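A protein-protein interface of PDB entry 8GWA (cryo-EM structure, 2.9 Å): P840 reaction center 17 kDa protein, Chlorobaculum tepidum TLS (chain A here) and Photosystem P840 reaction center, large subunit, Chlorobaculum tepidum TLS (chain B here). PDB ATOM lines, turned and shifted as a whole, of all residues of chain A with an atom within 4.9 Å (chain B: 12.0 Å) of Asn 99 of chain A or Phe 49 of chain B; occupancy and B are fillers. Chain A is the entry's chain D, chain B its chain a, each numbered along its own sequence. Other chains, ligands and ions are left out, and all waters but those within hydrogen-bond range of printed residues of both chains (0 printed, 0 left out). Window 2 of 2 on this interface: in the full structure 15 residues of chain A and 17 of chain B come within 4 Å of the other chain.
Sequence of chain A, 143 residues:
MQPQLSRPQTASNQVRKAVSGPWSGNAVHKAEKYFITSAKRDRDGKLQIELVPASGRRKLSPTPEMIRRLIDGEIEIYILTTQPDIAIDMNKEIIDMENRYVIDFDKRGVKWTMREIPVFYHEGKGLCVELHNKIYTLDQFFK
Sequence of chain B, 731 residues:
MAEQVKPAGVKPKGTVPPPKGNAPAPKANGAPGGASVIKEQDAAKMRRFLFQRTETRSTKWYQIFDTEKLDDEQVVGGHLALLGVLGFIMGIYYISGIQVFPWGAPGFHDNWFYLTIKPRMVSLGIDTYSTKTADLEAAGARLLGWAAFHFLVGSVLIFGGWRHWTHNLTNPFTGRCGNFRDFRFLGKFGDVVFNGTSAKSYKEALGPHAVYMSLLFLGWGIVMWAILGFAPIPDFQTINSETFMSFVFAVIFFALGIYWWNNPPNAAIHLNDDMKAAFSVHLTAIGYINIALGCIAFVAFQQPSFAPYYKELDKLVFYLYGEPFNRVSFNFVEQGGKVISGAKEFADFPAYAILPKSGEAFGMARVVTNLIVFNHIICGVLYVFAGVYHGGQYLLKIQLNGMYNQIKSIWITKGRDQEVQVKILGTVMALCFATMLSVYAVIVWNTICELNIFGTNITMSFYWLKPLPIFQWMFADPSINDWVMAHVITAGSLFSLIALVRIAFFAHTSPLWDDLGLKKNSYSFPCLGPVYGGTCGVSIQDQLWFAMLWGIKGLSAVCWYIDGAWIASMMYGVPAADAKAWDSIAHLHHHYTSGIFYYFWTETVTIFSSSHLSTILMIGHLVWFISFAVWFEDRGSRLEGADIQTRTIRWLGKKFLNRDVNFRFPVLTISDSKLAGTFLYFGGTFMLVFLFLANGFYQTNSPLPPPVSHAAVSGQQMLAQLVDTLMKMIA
O of Ile 95 of chain A sits close to ND2 of Asn 99 of chain A, at 3.3 Å. OE1 of Glu 98 of chain A is in hydrogen-bond range of OH of Tyr 101 of chain A (2.5 Å). O of Leu 50 of chain B sits at hydrogen-bond distance from OG1 of Thr 54 of chain B (2.9 Å).
The backbone carbonyl oxygen of Arg 100 of chain A sits at hydrogen-bond distance from the guanidinium group of Arg 53 of chain B, at 2.7 Å.
Among the printed residues, merely in contact across the chains: Arg 100 of chain A with Phe 49 of chain B, Tyr 101 of chain A with Thr 54 of chain B, Asn 99 of chain A with Leu 50 of chain B, Asn 99 of chain A with Phe 49 of chain B, Arg 100 of chain A with Leu 50 of chain B, Val 102 of chain A with Leu 50 of chain B, Tyr 101 of chain A with Leu 50 of chain B and Tyr 101 of chain A with Arg 53 of chain B.
Asn 99 of chain A touches just these residues of chain B: Phe 49 and Leu 50. Printed residues of chain A within 4 Å of Phe 49 of chain B: Asn 99 (3.4 Å) and Arg 100 (3.1 Å). Ile 95 of chain A touches none of the printed residues of chain B. No residue of chain B comes within 4 Å of Glu 98 of chain A. Tyr 101 of chain A touches three residues of chain B. Val 102 of chain A touches one residue of chain B. No residue of chain B comes within 4 Å of Val 110 of chain A. Of the printed residues of chain A, Leu 50 of chain B touches Asn 99, Arg 100, Tyr 101 and Val 102. Of the printed residues of chain A, Thr 54 of chain B touches Tyr 101. Printed residues of chain A within 4 Å of Arg 53 of chain B: Arg 100 and Tyr 101. Asp 104 of chain A touches none of the printed residues of chain B. The nearest residue of chain B that does not touch Asn 99 of chain A is Arg 53 of chain B (6.1 Å). The nearest residue of chain A that does not touch Phe 49 of chain B is Tyr 101 of chain A (4.8 Å). The nearest printed residue of chain A that does not touch Leu 50 of chain B is Glu 98 of chain A (4.9 Å).
Of the 10 printed residues of chain A, 4 touch a printed residue of chain B. Printed residues of chain A that touch a printed residue of chain B: Asn 99, Arg 100, Tyr 101 and Val 102. Hydrophobic or aromatic side chains of chain A within 4 Å of the printed part of chain B: Tyr 101. Among the printed residues, 9 pairs touch across the chains.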
ATOM      1  N   ILE A  95      18.213  -7.899 -16.659  1.00  0.00           N
ATOM      2  CA  ILE A  95      18.024  -9.157 -17.380  1.00  0.00           C
ATOM      3  C   ILE A  95      18.899 -10.257 -16.791  1.00  0.00           C
ATOM      4  O   ILE A  95      18.432 -11.375 -16.545  1.00  0.00           O
ATOM      5  CB  ILE A  95      18.293  -8.961 -18.883  1.00  0.00           C
ATOM      6  CG1 ILE A  95      17.059  -8.372 -19.568  1.00  0.00           C
ATOM      7  CG2 ILE A  95      18.682 -10.277 -19.539  1.00  0.00           C
ATOM      8  CD1 ILE A  95      17.240  -8.136 -21.050  1.00  0.00           C
ATOM      9  N   ASP A  96      20.177  -9.962 -16.548  1.00  0.00           N
ATOM     10  CA  ASP A  96      21.064 -10.993 -16.023  1.00  0.00           C
ATOM     11  C   ASP A  96      20.813 -11.288 -14.550  1.00  0.00           C
ATOM     12  O   ASP A  96      21.367 -12.261 -14.028  1.00  0.00           O
ATOM     13  CB  ASP A  96      22.530 -10.607 -16.252  1.00  0.00           C
ATOM     14  CG  ASP A  96      23.034  -9.561 -15.272  1.00  0.00           C
ATOM     15  OD1 ASP A  96      22.213  -8.816 -14.700  1.00  0.00           O
ATOM     16  OD2 ASP A  96      24.264  -9.485 -15.072  1.00  0.00           O
ATOM     17  N   MET A  97      19.998 -10.479 -13.873  1.00  0.00           N
ATOM     18  CA  MET A  97      19.612 -10.769 -12.500  1.00  0.00           C
ATOM     19  C   MET A  97      18.328 -11.579 -12.424  1.00  0.00           C
ATOM     20  O   MET A  97      18.155 -12.371 -11.490  1.00  0.00           O
ATOM     21  CB  MET A  97      19.457  -9.465 -11.713  1.00  0.00           C
ATOM     22  CG  MET A  97      19.176  -9.656 -10.237  1.00  0.00           C
ATOM     23  SD  MET A  97      20.561 -10.478  -9.436  1.00  0.00           S
ATOM     24  CE  MET A  97      21.771  -9.162  -9.438  1.00  0.00           C
ATOM     25  N   GLU A  98      17.428 -11.406 -13.393  1.00  0.00           N
ATOM     26  CA  GLU A  98      16.268 -12.278 -13.500  1.00  0.00           C
ATOM     27  C   GLU A  98      16.626 -13.642 -14.073  1.00  0.00           C
ATOM     28  O   GLU A  98      15.944 -14.624 -13.770  1.00  0.00           O
ATOM     29  CB  GLU A  98      15.185 -11.623 -14.359  1.00  0.00           C
ATOM     30  CG  GLU A  98      14.806 -10.215 -13.928  1.00  0.00           C
ATOM     31  CD  GLU A  98      14.059 -10.185 -12.608  1.00  0.00           C
ATOM     32  OE1 GLU A  98      13.142 -11.012 -12.424  1.00  0.00           O
ATOM     33  OE2 GLU A  98      14.389  -9.336 -11.754  1.00  0.00           O
ATOM     34  N   ASN A  99      17.697 -13.732 -14.862  1.00  0.00           N
ATOM     35  CA  ASN A  99      18.112 -15.019 -15.407  1.00  0.00           C
ATOM     36  C   ASN A  99      18.557 -15.990 -14.324  1.00  0.00           C
ATOM     37  O   ASN A  99      18.701 -17.185 -14.606  1.00  0.00           O
ATOM     38  CB  ASN A  99      19.238 -14.816 -16.420  1.00  0.00           C
ATOM     39  CG  ASN A  99      18.734 -14.307 -17.755  1.00  0.00           C
ATOM     40  OD1 ASN A  99      17.564 -14.477 -18.096  1.00  0.00           O
ATOM     41  ND2 ASN A  99      19.617 -13.676 -18.519  1.00  0.00           N
ATOM     42  N   ARG A 100      18.779 -15.506 -13.102  1.00  0.00           N
ATOM     43  CA  ARG A 100      19.116 -16.381 -11.987  1.00  0.00           C
ATOM     44  C   ARG A 100      17.910 -17.162 -11.484  1.00  0.00           C
ATOM     45  O   ARG A 100      18.069 -18.286 -10.997  1.00  0.00           O
ATOM     46  CB  ARG A 100      19.706 -15.560 -10.843  1.00  0.00           C
ATOM     47  CG  ARG A 100      20.976 -14.820 -11.203  1.00  0.00           C
ATOM     48  CD  ARG A 100      21.392 -13.862 -10.100  1.00  0.00           C
ATOM     49  NE  ARG A 100      21.922 -14.553  -8.930  1.00  0.00           N
ATOM     50  CZ  ARG A 100      21.220 -14.830  -7.841  1.00  0.00           C
ATOM     51  NH1 ARG A 100      19.948 -14.484  -7.731  1.00  0.00           N
ATOM     52  NH2 ARG A 100      21.810 -15.471  -6.836  1.00  0.00           N
ATOM     53  N   TYR A 101      16.706 -16.591 -11.583  1.00  0.00           N
ATOM     54  CA  TYR A 101      15.541 -17.210 -10.965  1.00  0.00           C
ATOM     55  C   TYR A 101      14.271 -17.136 -11.808  1.00  0.00           C
ATOM     56  O   TYR A 101      13.200 -17.490 -11.302  1.00  0.00           O
ATOM     57  CB  TYR A 101      15.272 -16.573  -9.596  1.00  0.00           C
ATOM     58  CG  TYR A 101      14.714 -15.170  -9.674  1.00  0.00           C
ATOM     59  CD1 TYR A 101      15.490 -14.116 -10.141  1.00  0.00           C
ATOM     60  CD2 TYR A 101      13.409 -14.901  -9.295  1.00  0.00           C
ATOM     61  CE1 TYR A 101      14.981 -12.835 -10.217  1.00  0.00           C
ATOM     62  CE2 TYR A 101      12.894 -13.623  -9.372  1.00  0.00           C
ATOM     63  CZ  TYR A 101      13.682 -12.595  -9.831  1.00  0.00           C
ATOM     64  OH  TYR A 101      13.166 -11.323  -9.904  1.00  0.00           O
ATOM     65  N   VAL A 102      14.341 -16.705 -13.065  1.00  0.00           N
ATOM     66  CA  VAL A 102      13.164 -16.591 -13.920  1.00  0.00           C
ATOM     67  C   VAL A 102      13.348 -17.500 -15.125  1.00  0.00           C
ATOM     68  O   VAL A 102      14.387 -17.449 -15.795  1.00  0.00           O
ATOM     69  CB  VAL A 102      12.913 -15.140 -14.376  1.00  0.00           C
ATOM     70  CG1 VAL A 102      11.576 -15.037 -15.092  1.00  0.00           C
ATOM     71  CG2 VAL A 102      12.966 -14.180 -13.201  1.00  0.00           C
ATOM     72  N   ASP A 104      11.873 -18.230 -18.809  1.00  0.00           N
ATOM     73  CA  ASP A 104      11.132 -17.489 -19.829  1.00  0.00           C
ATOM     74  C   ASP A 104      10.183 -18.431 -20.562  1.00  0.00           C
ATOM     75  O   ASP A 104      10.451 -18.910 -21.666  1.00  0.00           O
ATOM     76  CB  ASP A 104      12.091 -16.802 -20.791  1.00  0.00           C
ATOM     77  CG  ASP A 104      12.664 -15.524 -20.224  1.00  0.00           C
ATOM     78  OD1 ASP A 104      11.973 -14.883 -19.407  1.00  0.00           O
ATOM     79  OD2 ASP A 104      13.800 -15.162 -20.594  1.00  0.00           O
ATOM     80  N   VAL A 110      11.466 -11.329 -18.914  1.00  0.00           N
ATOM     81  CA  VAL A 110      12.698 -10.745 -18.393  1.00  0.00           C
ATOM     82  C   VAL A 110      13.096  -9.518 -19.204  1.00  0.00           C
ATOM     83  O   VAL A 110      13.587  -8.526 -18.654  1.00  0.00           O
ATOM     84  CB  VAL A 110      13.817 -11.803 -18.370  1.00  0.00           C
ATOM     85  CG1 VAL A 110      15.125 -11.183 -17.935  1.00  0.00           C
ATOM     86  CG2 VAL A 110      13.446 -12.934 -17.434  1.00  0.00           C
ATOM     87  N   ARG B  47      21.055 -24.433 -16.237  1.00  0.00           N
ATOM     88  CA  ARG B  47      19.637 -24.115 -16.102  1.00  0.00           C
ATOM     89  C   ARG B  47      19.016 -24.948 -14.988  1.00  0.00           C
ATOM     90  O   ARG B  47      17.857 -24.747 -14.624  1.00  0.00           O
ATOM     91  CB  ARG B  47      18.893 -24.362 -17.416  1.00  0.00           C
ATOM     92  CG  ARG B  47      18.596 -25.828 -17.696  1.00  0.00           C
ATOM     93  CD  ARG B  47      19.799 -26.560 -18.265  1.00  0.00           C
ATOM     94  NE  ARG B  47      19.444 -27.885 -18.758  1.00  0.00           N
ATOM     95  CZ  ARG B  47      20.323 -28.812 -19.111  1.00  0.00           C
ATOM     96  NH1 ARG B  47      21.626 -28.595 -19.031  1.00  0.00           N
ATOM     97  NH2 ARG B  47      19.884 -29.988 -19.551  1.00  0.00           N
ATOM     98  N   ARG B  48      19.796 -25.892 -14.455  1.00  0.00           N
ATOM     99  CA  ARG B  48      19.294 -26.755 -13.392  1.00  0.00           C
ATOM    100  C   ARG B  48      18.953 -25.956 -12.143  1.00  0.00           C
ATOM    101  O   ARG B  48      18.076 -26.357 -11.369  1.00  0.00           O
ATOM    102  CB  ARG B  48      20.321 -27.838 -13.064  1.00  0.00           C
ATOM    103  CG  ARG B  48      19.768 -28.990 -12.243  1.00  0.00           C
ATOM    104  CD  ARG B  48      20.877 -29.927 -11.797  1.00  0.00           C
ATOM    105  NE  ARG B  48      21.794 -29.281 -10.867  1.00  0.00           N
ATOM    106  CZ  ARG B  48      21.546 -29.099  -9.577  1.00  0.00           C
ATOM    107  NH1 ARG B  48      20.415 -29.507  -9.026  1.00  0.00           N
ATOM    108  NH2 ARG B  48      22.457 -28.495  -8.820  1.00  0.00           N
ATOM    109  N   PHE B  49      19.635 -24.830 -11.926  1.00  0.00           N
ATOM    110  CA  PHE B  49      19.286 -23.960 -10.810  1.00  0.00           C
ATOM    111  C   PHE B  49      17.888 -23.381 -10.980  1.00  0.00           C
ATOM    112  O   PHE B  49      17.109 -23.343 -10.021  1.00  0.00           O
ATOM    113  CB  PHE B  49      20.322 -22.841 -10.663  1.00  0.00           C
ATOM    114  CG  PHE B  49      20.444 -21.951 -11.871  1.00  0.00           C
ATOM    115  CD1 PHE B  49      21.146 -22.366 -12.990  1.00  0.00           C
ATOM    116  CD2 PHE B  49      19.864 -20.696 -11.880  1.00  0.00           C
ATOM    117  CE1 PHE B  49      21.260 -21.549 -14.096  1.00  0.00           C
ATOM    118  CE2 PHE B  49      19.975 -19.875 -12.983  1.00  0.00           C
ATOM    119  CZ  PHE B  49      20.674 -20.302 -14.093  1.00  0.00           C
ATOM    120  N   LEU B  50      17.543 -22.964 -12.203  1.00  0.00           N
ATOM    121  CA  LEU B  50      16.260 -22.311 -12.449  1.00  0.00           C
ATOM    122  C   LEU B  50      15.094 -23.183 -12.005  1.00  0.00           C
ATOM    123  O   LEU B  50      14.115 -22.682 -11.439  1.00  0.00           O
ATOM    124  CB  LEU B  50      16.125 -21.967 -13.932  1.00  0.00           C
ATOM    125  CG  LEU B  50      16.877 -20.739 -14.443  1.00  0.00           C
ATOM    126  CD1 LEU B  50      16.688 -20.584 -15.942  1.00  0.00           C
ATOM    127  CD2 LEU B  50      16.411 -19.495 -13.711  1.00  0.00           C
ATOM    128  N   PHE B  51      15.178 -24.489 -12.262  1.00  0.00           N
ATOM    129  CA  PHE B  51      14.114 -25.394 -11.844  1.00  0.00           C
ATOM    130  C   PHE B  51      13.970 -25.405 -10.328  1.00  0.00           C
ATOM    131  O   PHE B  51      12.852 -25.421  -9.802  1.00  0.00           O
ATOM    132  CB  PHE B  51      14.389 -26.798 -12.378  1.00  0.00           C
ATOM    133  CG  PHE B  51      14.627 -26.837 -13.859  1.00  0.00           C
ATOM    134  CD1 PHE B  51      13.674 -26.357 -14.739  1.00  0.00           C
ATOM    135  CD2 PHE B  51      15.808 -27.347 -14.371  1.00  0.00           C
ATOM    136  CE1 PHE B  51      13.893 -26.382 -16.100  1.00  0.00           C
ATOM    137  CE2 PHE B  51      16.031 -27.379 -15.734  1.00  0.00           C
ATOM    138  CZ  PHE B  51      15.072 -26.896 -16.600  1.00  0.00           C
ATOM    139  N   GLN B  52      15.094 -25.401  -9.609  1.00  0.00           N
ATOM    140  CA  GLN B  52      15.035 -25.299  -8.154  1.00  0.00           C
ATOM    141  C   GLN B  52      14.612 -23.903  -7.717  1.00  0.00           C
ATOM    142  O   GLN B  52      13.916 -23.748  -6.706  1.00  0.00           O
ATOM    143  CB  GLN B  52      16.386 -25.673  -7.547  1.00  0.00           C
ATOM    144  CG  GLN B  52      16.424 -25.599  -6.032  1.00  0.00           C
ATOM    145  CD  GLN B  52      17.726 -26.117  -5.462  1.00  0.00           C
ATOM    146  OE1 GLN B  52      18.444 -26.878  -6.112  1.00  0.00           O
ATOM    147  NE2 GLN B  52      18.037 -25.709  -4.239  1.00  0.00           N
ATOM    148  N   ARG B  53      15.031 -22.872  -8.458  1.00  0.00           N
ATOM    149  CA  ARG B  53      14.586 -21.514  -8.152  1.00  0.00           C
ATOM    150  C   ARG B  53      13.073 -21.394  -8.266  1.00  0.00           C
ATOM    151  O   ARG B  53      12.419 -20.836  -7.377  1.00  0.00           O
ATOM    152  CB  ARG B  53      15.258 -20.508  -9.091  1.00  0.00           C
ATOM    153  CG  ARG B  53      16.776 -20.509  -9.078  1.00  0.00           C
ATOM    154  CD  ARG B  53      17.321 -20.009  -7.766  1.00  0.00           C
ATOM    155  NE  ARG B  53      18.772 -20.117  -7.682  1.00  0.00           N
ATOM    156  CZ  ARG B  53      19.617 -19.166  -8.053  1.00  0.00           C
ATOM    157  NH1 ARG B  53      19.191 -18.015  -8.544  1.00  0.00           N
ATOM    158  NH2 ARG B  53      20.925 -19.375  -7.927  1.00  0.00           N
ATOM    159  N   THR B  54      12.502 -21.915  -9.347  1.00  0.00           N
ATOM    160  CA  THR B  54      11.072 -21.783  -9.625  1.00  0.00           C
ATOM    161  C   THR B  54      10.275 -22.969  -9.091  1.00  0.00           C
ATOM    162  O   THR B  54       9.516 -23.606  -9.821  1.00  0.00           O
ATOM    163  CB  THR B  54      10.855 -21.618 -11.124  1.00  0.00           C
ATOM    164  OG1 THR B  54      11.234 -22.826 -11.794  1.00  0.00           O
ATOM    165  CG2 THR B  54      11.702 -20.475 -11.658  1.00  0.00           C
ATOM    166  N   GLU B  55      10.439 -23.282  -7.810  1.00  0.00           N
ATOM    167  CA  GLU B  55       9.676 -24.340  -7.168  1.00  0.00           C
ATOM    168  C   GLU B  55       8.868 -23.781  -6.007  1.00  0.00           C
ATOM    169  O   GLU B  55       9.356 -22.956  -5.228  1.00  0.00           O
ATOM    170  CB  GLU B  55      10.580 -25.472  -6.665  1.00  0.00           C
ATOM    171  CG  GLU B  55      10.743 -26.621  -7.646  1.00  0.00           C
ATOM    172  CD  GLU B  55      11.777 -27.634  -7.196  1.00  0.00           C
ATOM    173  OE1 GLU B  55      11.972 -27.780  -5.972  1.00  0.00           O
ATOM    174  OE2 GLU B  55      12.392 -28.287  -8.065  1.00  0.00           O
ATOM    175  N   THR B  56       7.625 -24.238  -5.903  1.00  0.00           N
ATOM    176  CA  THR B  56       6.796 -23.928  -4.751  1.00  0.00           C
ATOM    177  C   THR B  56       7.366 -24.592  -3.506  1.00  0.00           C
ATOM    178  O   THR B  56       7.983 -25.660  -3.575  1.00  0.00           O
ATOM    179  CB  THR B  56       5.358 -24.395  -4.982  1.00  0.00           C
ATOM    180  OG1 THR B  56       4.947 -24.024  -6.304  1.00  0.00           O
ATOM    181  CG2 THR B  56       4.409 -23.768  -3.969  1.00  0.00           C
ATOM    182  N   LYS B 397       6.848 -32.171 -13.196  1.00  0.00           N
ATOM    183  CA  LYS B 397       8.274 -32.131 -12.892  1.00  0.00           C
ATOM    184  C   LYS B 397       9.112 -32.391 -14.137  1.00  0.00           C
ATOM    185  O   LYS B 397      10.122 -31.718 -14.368  1.00  0.00           O
ATOM    186  CB  LYS B 397       8.603 -33.147 -11.798  1.00  0.00           C
ATOM    187  CG  LYS B 397      10.018 -33.057 -11.258  1.00  0.00           C
ATOM    188  CD  LYS B 397      10.232 -34.052 -10.127  1.00  0.00           C
ATOM    189  CE  LYS B 397      11.555 -33.811  -9.419  1.00  0.00           C
ATOM    190  NZ  LYS B 397      11.518 -32.575  -8.589  1.00  0.00           N
ATOM    191  N   LEU B 400       8.672 -29.478 -16.798  1.00  0.00           N
ATOM    192  CA  LEU B 400       9.423 -28.275 -16.464  1.00  0.00           C
ATOM    193  C   LEU B 400      10.880 -28.403 -16.887  1.00  0.00           C
ATOM    194  O   LEU B 400      11.433 -27.500 -17.525  1.00  0.00           O
ATOM    195  CB  LEU B 400       9.316 -27.996 -14.965  1.00  0.00           C
ATOM    196  CG  LEU B 400       8.058 -27.259 -14.505  1.00  0.00           C
ATOM    197  CD1 LEU B 400       8.027 -27.137 -12.992  1.00  0.00           C
ATOM    198  CD2 LEU B 400       7.976 -25.891 -15.155  1.00  0.00           C
ATOM    199  N   ASN B 401      11.514 -29.528 -16.559  1.00  0.00           N
ATOM    200  CA  ASN B 401      12.933 -29.710 -16.835  1.00  0.00           C
ATOM    201  C   ASN B 401      13.220 -30.122 -18.274  1.00  0.00           C
ATOM    202  O   ASN B 401      14.392 -30.255 -18.640  1.00  0.00           O
ATOM    203  CB  ASN B 401      13.538 -30.720 -15.849  1.00  0.00           C
ATOM    204  CG  ASN B 401      12.925 -32.104 -15.962  1.00  0.00           C
ATOM    205  OD1 ASN B 401      12.303 -32.446 -16.964  1.00  0.00           O
ATOM    206  ND2 ASN B 401      13.104 -32.910 -14.923  1.00  0.00           N
ATOM    207  N   GLY B 402      12.188 -30.332 -19.092  1.00  0.00           N
ATOM    208  CA  GLY B 402      12.358 -30.492 -20.518  1.00  0.00           C
ATOM    209  C   GLY B 402      12.501 -31.912 -21.023  1.00  0.00           C
ATOM    210  O   GLY B 402      12.526 -32.112 -22.244  1.00  0.00           O
ATOM    211  N   ASN B 521       3.381 -24.238 -13.386  1.00  0.00           N
ATOM    212  CA  ASN B 521       4.698 -24.631 -12.899  1.00  0.00           C
ATOM    213  C   ASN B 521       4.718 -24.956 -11.408  1.00  0.00           C
ATOM    214  O   ASN B 521       5.794 -24.935 -10.798  1.00  0.00           O
ATOM    215  CB  ASN B 521       5.720 -23.529 -13.191  1.00  0.00           C
ATOM    216  CG  ASN B 521       5.227 -22.153 -12.786  1.00  0.00           C
ATOM    217  OD1 ASN B 521       4.386 -22.016 -11.896  1.00  0.00           O
ATOM    218  ND2 ASN B 521       5.746 -21.124 -13.441  1.00  0.00           N
